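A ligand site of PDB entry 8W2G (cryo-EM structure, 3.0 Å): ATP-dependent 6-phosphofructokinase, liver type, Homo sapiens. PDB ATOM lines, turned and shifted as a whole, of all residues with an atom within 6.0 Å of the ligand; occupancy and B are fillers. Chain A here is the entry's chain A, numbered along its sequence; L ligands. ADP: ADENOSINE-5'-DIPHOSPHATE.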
ATOM      1  N   ASN A 167      -7.294 -15.068 -27.495  1.00  0.00           N
ATOM      2  CA  ASN A 167      -5.881 -15.103 -27.863  1.00  0.00           C
ATOM      3  C   ASN A 167      -5.668 -14.488 -29.254  1.00  0.00           C
ATOM      4  O   ASN A 167      -5.018 -15.066 -30.120  1.00  0.00           O
ATOM      5  CB  ASN A 167      -5.320 -16.524 -27.783  1.00  0.00           C
ATOM      6  CG  ASN A 167      -3.823 -16.572 -27.577  1.00  0.00           C
ATOM      7  OD1 ASN A 167      -3.215 -15.650 -27.042  1.00  0.00           O
ATOM      8  ND2 ASN A 167      -3.215 -17.663 -28.001  1.00  0.00           N
ATOM      9  N   ASP A 173       1.924 -14.274 -26.914  1.00  0.00           N
ATOM     10  CA  ASP A 173       1.755 -15.660 -27.355  1.00  0.00           C
ATOM     11  C   ASP A 173       0.577 -16.323 -26.664  1.00  0.00           C
ATOM     12  O   ASP A 173      -0.068 -17.197 -27.254  1.00  0.00           O
ATOM     13  CB  ASP A 173       3.036 -16.459 -27.093  1.00  0.00           C
ATOM     14  CG  ASP A 173       4.206 -16.006 -27.941  1.00  0.00           C
ATOM     15  OD1 ASP A 173       4.008 -15.136 -28.819  1.00  0.00           O
ATOM     16  OD2 ASP A 173       5.325 -16.521 -27.738  1.00  0.00           O
ATOM     17  N   MET A 174       0.285 -15.946 -25.416  1.00  0.00           N
ATOM     18  CA  MET A 174      -0.860 -16.468 -24.677  1.00  0.00           C
ATOM     19  C   MET A 174      -1.475 -15.354 -23.842  1.00  0.00           C
ATOM     20  O   MET A 174      -0.803 -14.792 -22.972  1.00  0.00           O
ATOM     21  CB  MET A 174      -0.452 -17.632 -23.777  1.00  0.00           C
ATOM     22  CG  MET A 174      -0.180 -18.936 -24.508  1.00  0.00           C
ATOM     23  SD  MET A 174      -1.640 -19.659 -25.306  1.00  0.00           S
ATOM     24  CE  MET A 174      -2.054 -20.970 -24.158  1.00  0.00           C
ATOM     25  N   ASP A 179      -5.591 -20.898 -21.819  1.00  0.00           N
ATOM     26  CA  ASP A 179      -5.286 -22.305 -21.528  1.00  0.00           C
ATOM     27  C   ASP A 179      -6.420 -22.955 -20.767  1.00  0.00           C
ATOM     28  O   ASP A 179      -6.785 -24.100 -21.030  1.00  0.00           O
ATOM     29  CB  ASP A 179      -3.979 -22.406 -20.732  1.00  0.00           C
ATOM     30  CG  ASP A 179      -3.433 -23.823 -20.695  1.00  0.00           C
ATOM     31  OD1 ASP A 179      -3.063 -24.347 -21.756  1.00  0.00           O
ATOM     32  OD2 ASP A 179      -3.374 -24.397 -19.589  1.00  0.00           O
ATOM     33  N   TYR A 214      -8.005 -19.443 -32.948  1.00  0.00           N
ATOM     34  CA  TYR A 214      -7.011 -20.109 -32.110  1.00  0.00           C
ATOM     35  C   TYR A 214      -7.651 -21.231 -31.298  1.00  0.00           C
ATOM     36  O   TYR A 214      -7.141 -22.353 -31.269  1.00  0.00           O
ATOM     37  CB  TYR A 214      -6.337 -19.096 -31.183  1.00  0.00           C
ATOM     38  CG  TYR A 214      -5.195 -19.697 -30.374  1.00  0.00           C
ATOM     39  CD1 TYR A 214      -5.422 -20.292 -29.139  1.00  0.00           C
ATOM     40  CD2 TYR A 214      -3.888 -19.659 -30.852  1.00  0.00           C
ATOM     41  CE1 TYR A 214      -4.391 -20.857 -28.414  1.00  0.00           C
ATOM     42  CE2 TYR A 214      -2.854 -20.215 -30.125  1.00  0.00           C
ATOM     43  CZ  TYR A 214      -3.113 -20.816 -28.907  1.00  0.00           C
ATOM     44  OH  TYR A 214      -2.089 -21.358 -28.177  1.00  0.00           O
ATOM     45  N   VAL A 218      -6.649 -25.170 -31.867  1.00  0.00           N
ATOM     46  CA  VAL A 218      -5.982 -25.926 -30.821  1.00  0.00           C
ATOM     47  C   VAL A 218      -6.862 -27.061 -30.341  1.00  0.00           C
ATOM     48  O   VAL A 218      -6.397 -28.181 -30.117  1.00  0.00           O
ATOM     49  CB  VAL A 218      -5.581 -24.973 -29.664  1.00  0.00           C
ATOM     50  CG1 VAL A 218      -5.130 -25.729 -28.395  1.00  0.00           C
ATOM     51  CG2 VAL A 218      -4.452 -24.054 -30.133  1.00  0.00           C
ATOM     52  N   PHE A 308      -1.061 -23.299 -15.708  1.00  0.00           N
ATOM     53  CA  PHE A 308      -0.270 -22.356 -16.482  1.00  0.00           C
ATOM     54  C   PHE A 308      -0.844 -20.946 -16.405  1.00  0.00           C
ATOM     55  O   PHE A 308      -0.080 -19.969 -16.368  1.00  0.00           O
ATOM     56  CB  PHE A 308      -0.191 -22.793 -17.947  1.00  0.00           C
ATOM     57  CG  PHE A 308       0.476 -21.781 -18.834  1.00  0.00           C
ATOM     58  CD1 PHE A 308       1.835 -21.518 -18.694  1.00  0.00           C
ATOM     59  CD2 PHE A 308      -0.244 -21.084 -19.785  1.00  0.00           C
ATOM     60  CE1 PHE A 308       2.451 -20.584 -19.498  1.00  0.00           C
ATOM     61  CE2 PHE A 308       0.372 -20.150 -20.589  1.00  0.00           C
ATOM     62  CZ  PHE A 308       1.721 -19.895 -20.445  1.00  0.00           C
ATOM     63  N   LEU A 338       4.002 -12.545 -23.576  1.00  0.00           N
ATOM     64  CA  LEU A 338       4.888 -13.696 -23.778  1.00  0.00           C
ATOM     65  C   LEU A 338       5.657 -13.531 -25.075  1.00  0.00           C
ATOM     66  O   LEU A 338       5.064 -13.182 -26.107  1.00  0.00           O
ATOM     67  CB  LEU A 338       4.100 -15.014 -23.850  1.00  0.00           C
ATOM     68  CG  LEU A 338       3.657 -15.747 -22.588  1.00  0.00           C
ATOM     69  CD1 LEU A 338       4.834 -16.179 -21.719  1.00  0.00           C
ATOM     70  CD2 LEU A 338       2.701 -14.887 -21.837  1.00  0.00           C
ATOM     71  N   GLY A 340       8.658 -16.221 -26.695  1.00  0.00           N
ATOM     72  CA  GLY A 340       9.352 -17.432 -26.323  1.00  0.00           C
ATOM     73  C   GLY A 340       8.699 -18.050 -25.109  1.00  0.00           C
ATOM     74  O   GLY A 340       7.543 -18.498 -25.173  1.00  0.00           O
ATOM     75  N   ASN A 341       9.424 -18.074 -23.991  1.00  0.00           N
ATOM     76  CA  ASN A 341       8.890 -18.500 -22.708  1.00  0.00           C
ATOM     77  C   ASN A 341       9.451 -17.597 -21.614  1.00  0.00           C
ATOM     78  O   ASN A 341      10.023 -18.049 -20.620  1.00  0.00           O
ATOM     79  CB  ASN A 341       9.184 -19.979 -22.462  1.00  0.00           C
ATOM     80  CG  ASN A 341       8.558 -20.501 -21.189  1.00  0.00           C
ATOM     81  OD1 ASN A 341       7.365 -20.780 -21.138  1.00  0.00           O
ATOM     82  ND2 ASN A 341       9.372 -20.632 -20.158  1.00  0.00           N
ATOM     83  N   SER A 377       3.360 -19.466 -36.652  1.00  0.00           N
ATOM     84  CA  SER A 377       3.053 -20.623 -35.807  1.00  0.00           C
ATOM     85  C   SER A 377       1.642 -21.142 -36.071  1.00  0.00           C
ATOM     86  O   SER A 377       1.419 -22.356 -36.062  1.00  0.00           O
ATOM     87  CB  SER A 377       3.208 -20.246 -34.331  1.00  0.00           C
ATOM     88  OG  SER A 377       2.467 -19.073 -34.017  1.00  0.00           O
ATOM     89  N   ASN A 380       1.693 -23.188 -39.247  1.00  0.00           N
ATOM     90  CA  ASN A 380       2.341 -24.474 -39.039  1.00  0.00           C
ATOM     91  C   ASN A 380       1.416 -25.456 -38.323  1.00  0.00           C
ATOM     92  O   ASN A 380       1.349 -26.632 -38.698  1.00  0.00           O
ATOM     93  CB  ASN A 380       3.634 -24.279 -38.243  1.00  0.00           C
ATOM     94  CG  ASN A 380       4.406 -25.568 -38.067  1.00  0.00           C
ATOM     95  OD1 ASN A 380       4.280 -26.495 -38.860  1.00  0.00           O
ATOM     96  ND2 ASN A 380       5.218 -25.616 -37.017  1.00  0.00           N
ATOM     97  N   ASN A 381       0.685 -24.981 -37.316  1.00  0.00           N
ATOM     98  CA  ASN A 381      -0.283 -25.841 -36.640  1.00  0.00           C
ATOM     99  C   ASN A 381      -1.414 -26.230 -37.582  1.00  0.00           C
ATOM    100  O   ASN A 381      -1.906 -27.362 -37.535  1.00  0.00           O
ATOM    101  CB  ASN A 381      -0.840 -25.134 -35.400  1.00  0.00           C
ATOM    102  CG  ASN A 381       0.247 -24.678 -34.452  1.00  0.00           C
ATOM    103  OD1 ASN A 381       1.419 -25.040 -34.604  1.00  0.00           O
ATOM    104  ND2 ASN A 381      -0.131 -23.878 -33.453  1.00  0.00           N
ATOM    105  N   PHE A 537      10.479 -27.391 -21.492  1.00  0.00           N
ATOM    106  CA  PHE A 537       9.337 -28.168 -21.007  1.00  0.00           C
ATOM    107  C   PHE A 537       9.417 -29.581 -21.552  1.00  0.00           C
ATOM    108  O   PHE A 537       9.599 -29.779 -22.757  1.00  0.00           O
ATOM    109  CB  PHE A 537       8.016 -27.521 -21.434  1.00  0.00           C
ATOM    110  CG  PHE A 537       7.809 -26.157 -20.868  1.00  0.00           C
ATOM    111  CD1 PHE A 537       7.460 -25.984 -19.545  1.00  0.00           C
ATOM    112  CD2 PHE A 537       7.979 -25.038 -21.677  1.00  0.00           C
ATOM    113  CE1 PHE A 537       7.279 -24.714 -19.028  1.00  0.00           C
ATOM    114  CE2 PHE A 537       7.796 -23.777 -21.162  1.00  0.00           C
ATOM    115  CZ  PHE A 537       7.443 -23.614 -19.841  1.00  0.00           C
ATOM    116  N   ASP A 542       2.998 -30.457 -17.709  1.00  0.00           N
ATOM    117  CA  ASP A 542       1.811 -29.631 -17.489  1.00  0.00           C
ATOM    118  C   ASP A 542       0.680 -30.438 -16.850  1.00  0.00           C
ATOM    119  O   ASP A 542      -0.022 -29.931 -15.973  1.00  0.00           O
ATOM    120  CB  ASP A 542       1.344 -29.028 -18.815  1.00  0.00           C
ATOM    121  CG  ASP A 542       0.541 -27.761 -18.627  1.00  0.00           C
ATOM    122  OD1 ASP A 542       1.118 -26.772 -18.100  1.00  0.00           O
ATOM    123  OD2 ASP A 542      -0.642 -27.737 -19.000  1.00  0.00           O
ATOM    124  N   THR A 668      -3.548 -32.928 -20.565  1.00  0.00           N
ATOM    125  CA  THR A 668      -4.143 -31.621 -20.751  1.00  0.00           C
ATOM    126  C   THR A 668      -4.150 -31.297 -22.245  1.00  0.00           C
ATOM    127  O   THR A 668      -3.525 -32.003 -23.039  1.00  0.00           O
ATOM    128  CB  THR A 668      -3.358 -30.571 -19.957  1.00  0.00           C
ATOM    129  OG1 THR A 668      -1.996 -30.554 -20.379  1.00  0.00           O
ATOM    130  CG2 THR A 668      -3.428 -30.878 -18.469  1.00  0.00           C
ATOM    131  N   PHE A 670      -2.593 -28.893 -23.656  1.00  0.00           N
ATOM    132  CA  PHE A 670      -1.224 -28.543 -24.033  1.00  0.00           C
ATOM    133  C   PHE A 670      -0.387 -29.792 -24.302  1.00  0.00           C
ATOM    134  O   PHE A 670       0.351 -29.863 -25.283  1.00  0.00           O
ATOM    135  CB  PHE A 670      -0.575 -27.690 -22.946  1.00  0.00           C
ATOM    136  CG  PHE A 670       0.880 -27.436 -23.175  1.00  0.00           C
ATOM    137  CD1 PHE A 670       1.286 -26.489 -24.100  1.00  0.00           C
ATOM    138  CD2 PHE A 670       1.850 -28.139 -22.468  1.00  0.00           C
ATOM    139  CE1 PHE A 670       2.627 -26.244 -24.313  1.00  0.00           C
ATOM    140  CE2 PHE A 670       3.187 -27.903 -22.683  1.00  0.00           C
ATOM    141  CZ  PHE A 670       3.581 -26.951 -23.608  1.00  0.00           C
ATOM    142  N   TYR A 674       1.342 -30.461 -27.693  1.00  0.00           N
ATOM    143  CA  TYR A 674       2.796 -30.445 -27.605  1.00  0.00           C
ATOM    144  C   TYR A 674       3.383 -31.779 -28.026  1.00  0.00           C
ATOM    145  O   TYR A 674       4.368 -31.829 -28.768  1.00  0.00           O
ATOM    146  CB  TYR A 674       3.206 -30.080 -26.173  1.00  0.00           C
ATOM    147  CG  TYR A 674       4.668 -29.763 -25.951  1.00  0.00           C
ATOM    148  CD1 TYR A 674       5.292 -28.746 -26.657  1.00  0.00           C
ATOM    149  CD2 TYR A 674       5.412 -30.456 -25.005  1.00  0.00           C
ATOM    150  CE1 TYR A 674       6.617 -28.435 -26.442  1.00  0.00           C
ATOM    151  CE2 TYR A 674       6.741 -30.158 -24.786  1.00  0.00           C
ATOM    152  CZ  TYR A 674       7.338 -29.152 -25.502  1.00  0.00           C
ATOM    153  OH  TYR A 674       8.660 -28.850 -25.290  1.00  0.00           O
ATOM    154  N   LYS A 677       2.918 -32.040 -31.917  1.00  0.00           N
ATOM    155  CA  LYS A 677       3.872 -31.217 -32.646  1.00  0.00           C
ATOM    156  C   LYS A 677       5.275 -31.803 -32.593  1.00  0.00           C
ATOM    157  O   LYS A 677       5.991 -31.829 -33.601  1.00  0.00           O
ATOM    158  CB  LYS A 677       3.878 -29.797 -32.073  1.00  0.00           C
ATOM    159  CG  LYS A 677       2.705 -28.951 -32.501  1.00  0.00           C
ATOM    160  CD  LYS A 677       2.402 -27.906 -31.452  1.00  0.00           C
ATOM    161  CE  LYS A 677       1.442 -26.855 -31.957  1.00  0.00           C
ATOM    162  NZ  LYS A 677       0.659 -26.257 -30.845  1.00  0.00           N
ATOM    163  N   LYS A 681       7.543 -32.933 -35.819  1.00  0.00           N
ATOM    164  CA  LYS A 681       8.813 -32.243 -36.073  1.00  0.00           C
ATOM    165  C   LYS A 681      10.006 -33.181 -35.926  1.00  0.00           C
ATOM    166  O   LYS A 681      10.958 -33.101 -36.713  1.00  0.00           O
ATOM    167  CB  LYS A 681       8.964 -31.054 -35.141  1.00  0.00           C
ATOM    168  CG  LYS A 681       7.981 -29.940 -35.422  1.00  0.00           C
ATOM    169  CD  LYS A 681       8.161 -28.779 -34.459  1.00  0.00           C
ATOM    170  CE  LYS A 681       6.881 -27.979 -34.314  1.00  0.00           C
ATOM    171  NZ  LYS A 681       7.148 -26.533 -34.175  1.00  0.00           N
ATOM    172  N   LEU A 712      12.015 -27.661 -27.070  1.00  0.00           N
ATOM    173  CA  LEU A 712      11.605 -26.266 -27.252  1.00  0.00           C
ATOM    174  C   LEU A 712      12.510 -25.406 -26.379  1.00  0.00           C
ATOM    175  O   LEU A 712      12.397 -25.408 -25.159  1.00  0.00           O
ATOM    176  CB  LEU A 712      10.140 -26.096 -26.878  1.00  0.00           C
ATOM    177  CG  LEU A 712       9.374 -24.997 -27.633  1.00  0.00           C
ATOM    178  CD1 LEU A 712       9.138 -25.395 -29.087  1.00  0.00           C
ATOM    179  CD2 LEU A 712       8.057 -24.703 -26.943  1.00  0.00           C
HETATM  180  PB  ADP L   1       3.875 -23.094 -30.803  1.00  0.00           P
HETATM  181  O1B ADP L   1       4.139 -24.119 -31.879  1.00  0.00           O
HETATM  182  O2B ADP L   1       4.378 -23.611 -29.479  1.00  0.00           O
HETATM  183  O3B ADP L   1       4.574 -21.798 -31.153  1.00  0.00           O
HETATM  184  PA  ADP L   1       1.557 -21.730 -29.680  1.00  0.00           P
HETATM  185  O1A ADP L   1       0.055 -21.948 -29.670  1.00  0.00           O
HETATM  186  O2A ADP L   1       1.863 -20.328 -30.144  1.00  0.00           O
HETATM  187  O3A ADP L   1       2.246 -22.827 -30.697  1.00  0.00           O
HETATM  188  O5' ADP L   1       2.138 -21.943 -28.154  1.00  0.00           O
HETATM  189  C5' ADP L   1       2.035 -20.889 -27.247  1.00  0.00           C
HETATM  190  C4' ADP L   1       3.361 -20.745 -26.511  1.00  0.00           C
HETATM  191  O4' ADP L   1       3.126 -20.236 -25.079  1.00  0.00           O
HETATM  192  C3' ADP L   1       3.958 -21.969 -26.400  1.00  0.00           C
HETATM  193  O3' ADP L   1       5.035 -22.060 -27.329  1.00  0.00           O
HETATM  194  C2' ADP L   1       4.535 -22.080 -24.887  1.00  0.00           C
HETATM  195  O2' ADP L   1       5.870 -21.541 -24.824  1.00  0.00           O
HETATM  196  C1' ADP L   1       3.727 -21.360 -24.119  1.00  0.00           C
HETATM  197  N9  ADP L   1       2.674 -22.168 -23.586  1.00  0.00           N
HETATM  198  C8  ADP L   1       1.425 -22.179 -24.035  1.00  0.00           C
HETATM  199  N7  ADP L   1       0.715 -23.029 -23.317  1.00  0.00           N
HETATM  200  C5  ADP L   1       1.497 -23.560 -22.377  1.00  0.00           C
HETATM  201  C6  ADP L   1       1.296 -24.504 -21.349  1.00  0.00           C
HETATM  202  N6  ADP L   1      -0.009 -25.096 -21.140  1.00  0.00           N
HETATM  203  N1  ADP L   1       2.330 -24.818 -20.589  1.00  0.00           N
HETATM  204  C2  ADP L   1       3.529 -24.284 -20.772  1.00  0.00           C
HETATM  205  N3  ADP L   1       3.744 -23.395 -21.724  1.00  0.00           N
HETATM  206  C4  ADP L   1       2.752 -23.015 -22.547  1.00  0.00           C
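OH of Tyr 214 lies within hydrogen-bond range of O1A of the ligand, at 2.7 Å.
N6 of the ligand lies within hydrogen-bond range of OD1 of Asp 179 (3.2 Å).
OD2 of Asp 542 is in hydrogen-bond range of N6 of the ligand (3.5 Å).
O2' of the ligand lies within hydrogen-bond range of O of Gly 340.
The side-chain hydroxyl of Tyr 214 sits at hydrogen-bond distance from the side-chain sulfur of Met 174 (3.4 Å).
The side-chain carboxylate (OD2) of Asp 542 lies within hydrogen-bond range of the side-chain hydroxyl (OG1) of Thr 668, 3.4 Å away.
SD of Met 174 lies within hydrogen-bond range of ND2 of Asn 167 (3.7 Å).
OD1 of Asn 381 sits close to O of Ser 377 (3.1 Å).
Residues that only touch the ligand: Met 174 (3.6 Å), Phe 308 (3.8 Å), Ser 377 (3.8 Å), Asn 381 (3.8 Å), Phe 670 (3.2 Å) and Lys 677 (3.8 Å).
Hydrophobic or aromatic side chains within 4 Å of the ligand: Met 174, Tyr 214, Phe 308 and Phe 670.
Of the 21 residues printed, 10 come within 4 Å of the ligand.
The nearest printed residue that does not touch the ligand is Leu 712 (4.03 Å).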
